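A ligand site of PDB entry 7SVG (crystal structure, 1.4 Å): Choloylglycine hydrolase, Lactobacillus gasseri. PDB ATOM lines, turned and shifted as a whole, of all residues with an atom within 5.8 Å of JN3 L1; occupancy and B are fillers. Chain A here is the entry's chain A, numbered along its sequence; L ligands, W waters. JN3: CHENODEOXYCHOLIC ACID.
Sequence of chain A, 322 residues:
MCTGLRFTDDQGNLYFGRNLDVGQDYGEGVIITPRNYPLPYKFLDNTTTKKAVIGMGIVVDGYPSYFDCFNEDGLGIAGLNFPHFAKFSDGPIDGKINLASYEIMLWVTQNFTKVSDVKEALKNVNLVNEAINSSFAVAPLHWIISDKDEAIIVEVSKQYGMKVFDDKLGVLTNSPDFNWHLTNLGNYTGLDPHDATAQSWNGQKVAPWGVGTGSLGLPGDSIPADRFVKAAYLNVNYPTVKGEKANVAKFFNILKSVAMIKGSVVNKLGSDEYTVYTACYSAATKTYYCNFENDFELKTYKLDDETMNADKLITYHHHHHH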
ATOM      1  N   OCS A   2     -12.730  28.195  11.255  1.00  0.00           N
ATOM      2  CA  OCS A   2     -14.057  27.593  11.115  1.00  0.00           C
ATOM      3  CB  OCS A   2     -15.081  28.236  12.067  1.00  0.00           C
ATOM      4  SG  OCS A   2     -14.610  28.384  13.783  1.00  0.00           S
ATOM      5  C   OCS A   2     -14.619  27.753   9.705  1.00  0.00           C
ATOM      6  O   OCS A   2     -14.345  28.754   9.026  1.00  0.00           O
ATOM      7  OD1 OCS A   2     -13.870  29.584  13.948  1.00  0.00           O
ATOM      8  OD2 OCS A   2     -15.808  28.531  14.543  1.00  0.00           O
ATOM      9  OD3 OCS A   2     -13.891  27.252  14.228  1.00  0.00           O
ATOM     10  N   ARG A  18     -20.954  22.727  10.209  1.00  0.00           N
ATOM     11  CA  ARG A  18     -19.715  23.503  10.317  1.00  0.00           C
ATOM     12  C   ARG A  18     -18.545  22.627  10.737  1.00  0.00           C
ATOM     13  O   ARG A  18     -18.715  21.557  11.319  1.00  0.00           O
ATOM     14  CB  ARG A  18     -19.882  24.660  11.324  1.00  0.00           C
ATOM     15  CG  ARG A  18     -20.277  24.203  12.744  1.00  0.00           C
ATOM     16  CD  ARG A  18     -19.057  23.992  13.679  1.00  0.00           C
ATOM     17  NE  ARG A  18     -18.324  25.218  13.923  1.00  0.00           N
ATOM     18  CZ  ARG A  18     -18.782  26.198  14.699  1.00  0.00           C
ATOM     19  NH1 ARG A  18     -19.927  26.086  15.356  1.00  0.00           N
ATOM     20  NH2 ARG A  18     -18.085  27.331  14.793  1.00  0.00           N
ATOM     21  N   LEU A  20     -15.357  23.156  13.364  1.00  0.00           N
ATOM     22  CA  LEU A  20     -14.841  23.988  14.453  1.00  0.00           C
ATOM     23  C   LEU A  20     -13.326  23.900  14.398  1.00  0.00           C
ATOM     24  O   LEU A  20     -12.750  22.823  14.617  1.00  0.00           O
ATOM     25  CB  LEU A  20     -15.362  23.537  15.822  1.00  0.00           C
ATOM     26  CG  LEU A  20     -14.779  24.409  16.934  1.00  0.00           C
ATOM     27  CD1 LEU A  20     -15.320  25.847  16.857  1.00  0.00           C
ATOM     28  CD2 LEU A  20     -15.029  23.830  18.317  1.00  0.00           C
ATOM     29  N   ASP A  21     -12.672  25.033  14.109  1.00  0.00           N
ATOM     30  CA  ASP A  21     -11.216  25.091  13.962  1.00  0.00           C
ATOM     31  C   ASP A  21     -10.657  25.896  15.123  1.00  0.00           C
ATOM     32  O   ASP A  21     -10.911  27.101  15.220  1.00  0.00           O
ATOM     33  CB  ASP A  21     -10.798  25.711  12.626  1.00  0.00           C
ATOM     34  CG  ASP A  21     -11.397  25.011  11.429  1.00  0.00           C
ATOM     35  OD1 ASP A  21     -11.921  23.885  11.588  1.00  0.00           O
ATOM     36  OD2 ASP A  21     -11.347  25.591  10.333  1.00  0.00           O
ATOM     37  N   VAL A  22      -9.896  25.244  16.008  1.00  0.00           N
ATOM     38  CA  VAL A  22      -9.471  25.862  17.250  1.00  0.00           C
ATOM     39  C   VAL A  22      -8.104  25.314  17.649  1.00  0.00           C
ATOM     40  O   VAL A  22      -7.598  24.349  17.074  1.00  0.00           O
ATOM     41  CB  VAL A  22     -10.499  25.651  18.381  1.00  0.00           C
ATOM     42  CG1 VAL A  22     -11.755  26.464  18.105  1.00  0.00           C
ATOM     43  CG2 VAL A  22     -10.825  24.181  18.526  1.00  0.00           C
ATOM     44  N   TYR A  26     -12.312  22.176  24.004  1.00  0.00           N
ATOM     45  CA  TYR A  26     -12.956  22.940  25.063  1.00  0.00           C
ATOM     46  C   TYR A  26     -13.896  22.101  25.926  1.00  0.00           C
ATOM     47  O   TYR A  26     -14.603  22.654  26.772  1.00  0.00           O
ATOM     48  CB  TYR A  26     -13.694  24.155  24.492  1.00  0.00           C
ATOM     49  CG  TYR A  26     -12.760  25.192  23.876  1.00  0.00           C
ATOM     50  CD1 TYR A  26     -12.057  26.081  24.686  1.00  0.00           C
ATOM     51  CD2 TYR A  26     -12.580  25.271  22.501  1.00  0.00           C
ATOM     52  CE1 TYR A  26     -11.201  27.029  24.136  1.00  0.00           C
ATOM     53  CE2 TYR A  26     -11.718  26.217  21.938  1.00  0.00           C
ATOM     54  CZ  TYR A  26     -11.036  27.096  22.757  1.00  0.00           C
ATOM     55  OH  TYR A  26     -10.188  28.038  22.204  1.00  0.00           O
ATOM     56  N   TYR A  66     -24.574  27.094  23.070  1.00  0.00           N
ATOM     57  CA  TYR A  66     -24.310  26.360  21.829  1.00  0.00           C
ATOM     58  C   TYR A  66     -23.259  27.029  20.953  1.00  0.00           C
ATOM     59  O   TYR A  66     -23.270  28.257  20.772  1.00  0.00           O
ATOM     60  CB  TYR A  66     -25.609  26.224  21.028  1.00  0.00           C
ATOM     61  CG  TYR A  66     -26.543  25.127  21.505  1.00  0.00           C
ATOM     62  CD1 TYR A  66     -26.247  23.788  21.254  1.00  0.00           C
ATOM     63  CD2 TYR A  66     -27.721  25.418  22.186  1.00  0.00           C
ATOM     64  CE1 TYR A  66     -27.087  22.780  21.663  1.00  0.00           C
ATOM     65  CE2 TYR A  66     -28.575  24.392  22.601  1.00  0.00           C
ATOM     66  CZ  TYR A  66     -28.251  23.088  22.340  1.00  0.00           C
ATOM     67  OH  TYR A  66     -29.081  22.045  22.721  1.00  0.00           O
ATOM     68  N   PHE A  67     -22.376  26.211  20.377  1.00  0.00           N
ATOM     69  CA  PHE A  67     -21.501  26.656  19.293  1.00  0.00           C
ATOM     70  C   PHE A  67     -22.240  26.663  17.962  1.00  0.00           C
ATOM     71  O   PHE A  67     -21.936  27.473  17.069  1.00  0.00           O
ATOM     72  CB  PHE A  67     -20.329  25.674  19.132  1.00  0.00           C
ATOM     73  CG  PHE A  67     -19.437  25.520  20.347  1.00  0.00           C
ATOM     74  CD1 PHE A  67     -19.725  26.115  21.570  1.00  0.00           C
ATOM     75  CD2 PHE A  67     -18.282  24.753  20.244  1.00  0.00           C
ATOM     76  CE1 PHE A  67     -18.887  25.938  22.669  1.00  0.00           C
ATOM     77  CE2 PHE A  67     -17.437  24.570  21.339  1.00  0.00           C
ATOM     78  CZ  PHE A  67     -17.747  25.163  22.552  1.00  0.00           C
ATOM     79  N   ASP A  68     -23.186  25.745  17.793  1.00  0.00           N
ATOM     80  CA  ASP A  68     -24.097  25.623  16.673  1.00  0.00           C
ATOM     81  C   ASP A  68     -25.372  24.979  17.228  1.00  0.00           C
ATOM     82  O   ASP A  68     -25.299  24.213  18.193  1.00  0.00           O
ATOM     83  CB  ASP A  68     -23.471  24.843  15.498  1.00  0.00           C
ATOM     84  CG  ASP A  68     -22.702  23.633  15.957  1.00  0.00           C
ATOM     85  OD1 ASP A  68     -23.340  22.602  16.259  1.00  0.00           O
ATOM     86  OD2 ASP A  68     -21.453  23.711  15.939  1.00  0.00           O
ATOM     87  N   ALA A  78     -25.022  28.892  13.367  1.00  0.00           N
ATOM     88  CA  ALA A  78     -23.708  28.522  13.876  1.00  0.00           C
ATOM     89  C   ALA A  78     -22.924  29.793  14.136  1.00  0.00           C
ATOM     90  O   ALA A  78     -22.967  30.723  13.321  1.00  0.00           O
ATOM     91  CB  ALA A  78     -22.939  27.646  12.863  1.00  0.00           C
ATOM     92  N   GLY A  79     -22.225  29.843  15.265  1.00  0.00           N
ATOM     93  CA  GLY A  79     -21.362  30.966  15.603  1.00  0.00           C
ATOM     94  C   GLY A  79     -19.905  30.640  15.310  1.00  0.00           C
ATOM     95  O   GLY A  79     -19.363  29.661  15.844  1.00  0.00           O
ATOM     96  N   LEU A  80     -19.283  31.455  14.478  1.00  0.00           N
ATOM     97  CA  LEU A  80     -17.921  31.249  14.018  1.00  0.00           C
ATOM     98  C   LEU A  80     -17.079  32.449  14.427  1.00  0.00           C
ATOM     99  O   LEU A  80     -17.582  33.556  14.592  1.00  0.00           O
ATOM    100  CB  LEU A  80     -17.883  31.110  12.488  1.00  0.00           C
ATOM    101  CG  LEU A  80     -18.317  29.759  11.892  1.00  0.00           C
ATOM    102  CD1 LEU A  80     -19.788  29.448  12.100  1.00  0.00           C
ATOM    103  CD2 LEU A  80     -17.977  29.711  10.409  1.00  0.00           C
ATOM    104  N   ASN A  81     -15.765  32.211  14.566  1.00  0.00           N
ATOM    105  CA  ASN A  81     -14.874  33.267  15.048  1.00  0.00           C
ATOM    106  C   ASN A  81     -14.821  34.426  14.064  1.00  0.00           C
ATOM    107  O   ASN A  81     -14.803  34.231  12.843  1.00  0.00           O
ATOM    108  CB  ASN A  81     -13.475  32.686  15.262  1.00  0.00           C
ATOM    109  CG  ASN A  81     -12.690  33.420  16.335  1.00  0.00           C
ATOM    110  OD1 ASN A  81     -13.263  33.912  17.317  1.00  0.00           O
ATOM    111  ND2 ASN A  81     -11.364  33.495  16.164  1.00  0.00           N
ATOM    112  N   PHE A  82     -14.770  35.641  14.602  1.00  0.00           N
ATOM    113  CA  PHE A  82     -14.748  36.867  13.797  1.00  0.00           C
ATOM    114  C   PHE A  82     -13.804  37.858  14.465  1.00  0.00           C
ATOM    115  O   PHE A  82     -14.190  38.971  14.809  1.00  0.00           O
ATOM    116  CB  PHE A  82     -16.184  37.396  13.716  1.00  0.00           C
ATOM    117  CG  PHE A  82     -16.420  38.482  12.683  1.00  0.00           C
ATOM    118  CD1 PHE A  82     -15.726  38.521  11.483  1.00  0.00           C
ATOM    119  CD2 PHE A  82     -17.384  39.461  12.932  1.00  0.00           C
ATOM    120  CE1 PHE A  82     -16.001  39.524  10.548  1.00  0.00           C
ATOM    121  CE2 PHE A  82     -17.657  40.451  12.024  1.00  0.00           C
ATOM    122  CZ  PHE A  82     -16.963  40.491  10.824  1.00  0.00           C
ATOM    123  N   ALA A 137     -15.310  35.199  29.237  1.00  0.00           N
ATOM    124  CA  ALA A 137     -15.052  36.141  28.166  1.00  0.00           C
ATOM    125  C   ALA A 137     -16.206  36.125  27.175  1.00  0.00           C
ATOM    126  O   ALA A 137     -16.896  35.119  27.006  1.00  0.00           O
ATOM    127  CB  ALA A 137     -13.759  35.770  27.426  1.00  0.00           C
ATOM    128  N   VAL A 138     -16.400  37.242  26.494  1.00  0.00           N
ATOM    129  CA  VAL A 138     -17.353  37.303  25.386  1.00  0.00           C
ATOM    130  C   VAL A 138     -16.650  36.808  24.126  1.00  0.00           C
ATOM    131  O   VAL A 138     -15.545  37.251  23.804  1.00  0.00           O
ATOM    132  CB  VAL A 138     -17.856  38.742  25.185  1.00  0.00           C
ATOM    133  CG1 VAL A 138     -18.697  38.832  23.902  1.00  0.00           C
ATOM    134  CG2 VAL A 138     -18.654  39.200  26.416  1.00  0.00           C
ATOM    135  N   ALA A 139     -17.302  35.894  23.399  1.00  0.00           N
ATOM    136  CA  ALA A 139     -16.688  35.376  22.180  1.00  0.00           C
ATOM    137  C   ALA A 139     -16.885  36.352  21.026  1.00  0.00           C
ATOM    138  O   ALA A 139     -18.007  36.833  20.815  1.00  0.00           O
ATOM    139  CB  ALA A 139     -17.303  34.038  21.828  1.00  0.00           C
ATOM    140  N   PRO A 140     -15.852  36.634  20.248  1.00  0.00           N
ATOM    141  CA  PRO A 140     -15.982  37.600  19.127  1.00  0.00           C
ATOM    142  C   PRO A 140     -16.486  36.891  17.872  1.00  0.00           C
ATOM    143  O   PRO A 140     -15.727  36.512  16.981  1.00  0.00           O
ATOM    144  CB  PRO A 140     -14.536  38.086  18.947  1.00  0.00           C
ATOM    145  CG  PRO A 140     -13.687  36.854  19.344  1.00  0.00           C
ATOM    146  CD  PRO A 140     -14.493  36.119  20.409  1.00  0.00           C
ATOM    147  N   LEU A 141     -17.793  36.647  17.797  1.00  0.00           N
ATOM    148  CA  LEU A 141     -18.382  35.780  16.776  1.00  0.00           C
ATOM    149  C   LEU A 141     -19.119  36.566  15.696  1.00  0.00           C
ATOM    150  O   LEU A 141     -19.507  37.725  15.873  1.00  0.00           O
ATOM    151  CB  LEU A 141     -19.385  34.798  17.413  1.00  0.00           C
ATOM    152  CG  LEU A 141     -18.847  33.980  18.564  1.00  0.00           C
ATOM    153  CD1 LEU A 141     -19.912  33.034  19.080  1.00  0.00           C
ATOM    154  CD2 LEU A 141     -17.615  33.198  18.081  1.00  0.00           C
HETATM  155  C1  JN3 L   1     -16.985  28.842  21.409  1.00  0.00           C
HETATM  156  C2  JN3 L   1     -18.088  29.650  20.740  1.00  0.00           C
HETATM  157  C3  JN3 L   1     -18.356  29.108  19.353  1.00  0.00           C
HETATM  158  O3  JN3 L   1     -19.456  29.733  18.709  1.00  0.00           O
HETATM  159  C4  JN3 L   1     -17.109  29.341  18.510  1.00  0.00           C
HETATM  160  C5  JN3 L   1     -15.822  28.735  19.111  1.00  0.00           C
HETATM  161  C6  JN3 L   1     -14.550  29.127  18.307  1.00  0.00           C
HETATM  162  C7  JN3 L   1     -13.896  30.459  18.685  1.00  0.00           C
HETATM  163  O7  JN3 L   1     -14.717  31.531  18.211  1.00  0.00           O
HETATM  164  C8  JN3 L   1     -13.658  30.600  20.200  1.00  0.00           C
HETATM  165  C9  JN3 L   1     -14.992  30.361  20.948  1.00  0.00           C
HETATM  166  C10 JN3 L   1     -15.631  28.951  20.654  1.00  0.00           C
HETATM  167  C11 JN3 L   1     -14.881  30.647  22.465  1.00  0.00           C
HETATM  168  C12 JN3 L   1     -14.282  32.011  22.797  1.00  0.00           C
HETATM  169  C13 JN3 L   1     -12.896  32.144  22.138  1.00  0.00           C
HETATM  170  C14 JN3 L   1     -13.135  31.973  20.621  1.00  0.00           C
HETATM  171  C15 JN3 L   1     -11.811  32.399  19.993  1.00  0.00           C
HETATM  172  C16 JN3 L   1     -11.318  33.521  20.909  1.00  0.00           C
HETATM  173  C17 JN3 L   1     -12.334  33.577  22.085  1.00  0.00           C
HETATM  174  C18 JN3 L   1     -11.899  31.135  22.746  1.00  0.00           C
HETATM  175  C19 JN3 L   1     -14.724  27.830  21.208  1.00  0.00           C
HETATM  176  C20 JN3 L   1     -11.752  34.199  23.336  1.00  0.00           C
HETATM  177  C21 JN3 L   1     -12.466  33.751  24.614  1.00  0.00           C
HETATM  178  C22 JN3 L   1     -11.927  35.728  23.145  1.00  0.00           C
HETATM  179  C23 JN3 L   1     -10.643  36.516  22.988  1.00  0.00           C
HETATM  180  O25 JN3 L   1     -11.818  38.575  22.232  1.00  0.00           O
HETATM  181  C24 JN3 L   1     -10.807  37.871  22.327  1.00  0.00           C
HETATM  182  O26 JN3 L   1      -9.597  38.251  21.844  1.00  0.00           O
HETATM  183  C1  JN3 L   2     -20.662  30.086  26.605  1.00  0.00           C
HETATM  184  C2  JN3 L   2     -20.973  30.968  27.797  1.00  0.00           C
HETATM  185  C3  JN3 L   2     -20.915  32.420  27.381  1.00  0.00           C
HETATM  186  O3  JN3 L   2     -21.223  33.276  28.462  1.00  0.00           O
HETATM  187  C4  JN3 L   2     -19.512  32.763  26.907  1.00  0.00           C
HETATM  188  C5  JN3 L   2     -19.112  31.934  25.675  1.00  0.00           C
HETATM  189  C6  JN3 L   2     -17.710  32.333  25.182  1.00  0.00           C
HETATM  190  C7  JN3 L   2     -16.572  31.741  26.004  1.00  0.00           C
HETATM  191  O7  JN3 L   2     -16.487  32.414  27.260  1.00  0.00           O
HETATM  192  C8  JN3 L   2     -16.737  30.225  26.201  1.00  0.00           C
HETATM  193  C9  JN3 L   2     -18.112  29.873  26.824  1.00  0.00           C
HETATM  194  C10 JN3 L   2     -19.293  30.403  25.922  1.00  0.00           C
HETATM  195  C11 JN3 L   2     -18.174  28.360  27.123  1.00  0.00           C
HETATM  196  C12 JN3 L   2     -16.969  27.798  27.907  1.00  0.00           C
HETATM  197  C13 JN3 L   2     -15.662  28.097  27.167  1.00  0.00           C
HETATM  198  C14 JN3 L   2     -15.604  29.631  27.044  1.00  0.00           C
HETATM  199  C15 JN3 L   2     -14.184  29.945  26.598  1.00  0.00           C
HETATM  200  C16 JN3 L   2     -13.346  28.840  27.244  1.00  0.00           C
HETATM  201  C17 JN3 L   2     -14.348  27.904  27.968  1.00  0.00           C
HETATM  202  C18 JN3 L   2     -15.635  27.328  25.822  1.00  0.00           C
HETATM  203  C19 JN3 L   2     -19.347  29.691  24.545  1.00  0.00           C
HETATM  204  C20 JN3 L   2     -13.832  26.479  28.087  1.00  0.00           C
HETATM  205  C21 JN3 L   2     -14.907  25.595  28.721  1.00  0.00           C
HETATM  206  C22 JN3 L   2     -12.506  26.452  28.865  1.00  0.00           C
HETATM  207  C23 JN3 L   2     -11.770  25.117  28.682  1.00  0.00           C
HETATM  208  O25 JN3 L   2     -10.590  24.614  30.747  1.00  0.00           O
HETATM  209  C24 JN3 L   2     -10.568  25.000  29.585  1.00  0.00           C
HETATM  210  O26 JN3 L   2      -9.428  25.387  28.957  1.00  0.00           O
HETATM  211  O   HOH W   1      -9.631  36.924  19.194  1.00  0.00           O
HETATM  212  O   HOH W   2     -14.629  39.499  22.557  1.00  0.00           O
HETATM  213  O   HOH W   3     -21.760  30.354  20.017  1.00  0.00           O
HETATM  214  O   HOH W   4     -12.046  29.493  15.987  1.00  0.00           O
HETATM  215  O   HOH W   5      -8.049  38.967  18.972  1.00  0.00           O
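The backbone carbonyl oxygen (O) of Gly 79 is in hydrogen-bond range of an oxygen (O3) of JN3 L1.
The side-chain amide oxygen (OD1) of Asn 81 sits at hydrogen-bond distance from an oxygen (O7) of JN3 L1 (2.9 Å).
The backbone carbonyl oxygen of Ala 137 lies within hydrogen-bond range of an oxygen (O7) of JN3 L2 (2.7 Å).
The backbone NH (N) of Gly 79 sits at hydrogen-bond distance from the backbone carbonyl oxygen (O) of Phe 67 (3.0 Å).
NH2 of Arg 18 sits at hydrogen-bond distance from O of Gly 79.
N of Asn 81 sits at hydrogen-bond distance from OD1 of OCS 2 (3.3 Å).
The backbone carbonyl oxygen (O) of Phe 67 lies within hydrogen-bond range of the guanidinium group (NH1) of Arg 18, 3.0 Å away.
The backbone carbonyl oxygen of Pro 140 lies within hydrogen-bond range of the backbone NH of Phe 82, at 2.7 Å.
Residues that only touch JN3 L1: Leu 141, Tyr 26, Leu 20, Phe 67, Ala 137, Pro 140, Ala 139, Val 22 and Val 138.
Hydrophobic or aromatic side chains within 4 Å of JN3 L1: Leu 20, Val 22, Tyr 26, Phe 67, Ala 137, Ala 139, Pro 140 and Leu 141.
11 residues have an atom within 4 Å of JN3 L1: Leu 20, Val 22, Tyr 26, Phe 67, Gly 79, Asn 81, Ala 137, Val 138, Ala 139, Pro 140 and Leu 141.
Water W3 lies within hydrogen-bond range of the backbone carbonyl oxygen (O) of Tyr 66 (2.7 Å) and an oxygen (O3) of JN3 L1 (2.7 Å).
Water W2 lies within hydrogen-bond range of the backbone carbonyl oxygen (O) of Val 138 (2.7 Å) and an oxygen (O25) of JN3 L1 (3.0 Å).
Water W4 bridges OD1 of OCS 2 (2.7 Å) and the backbone carbonyl oxygen (O) of Asp 21 (2.8 Å).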
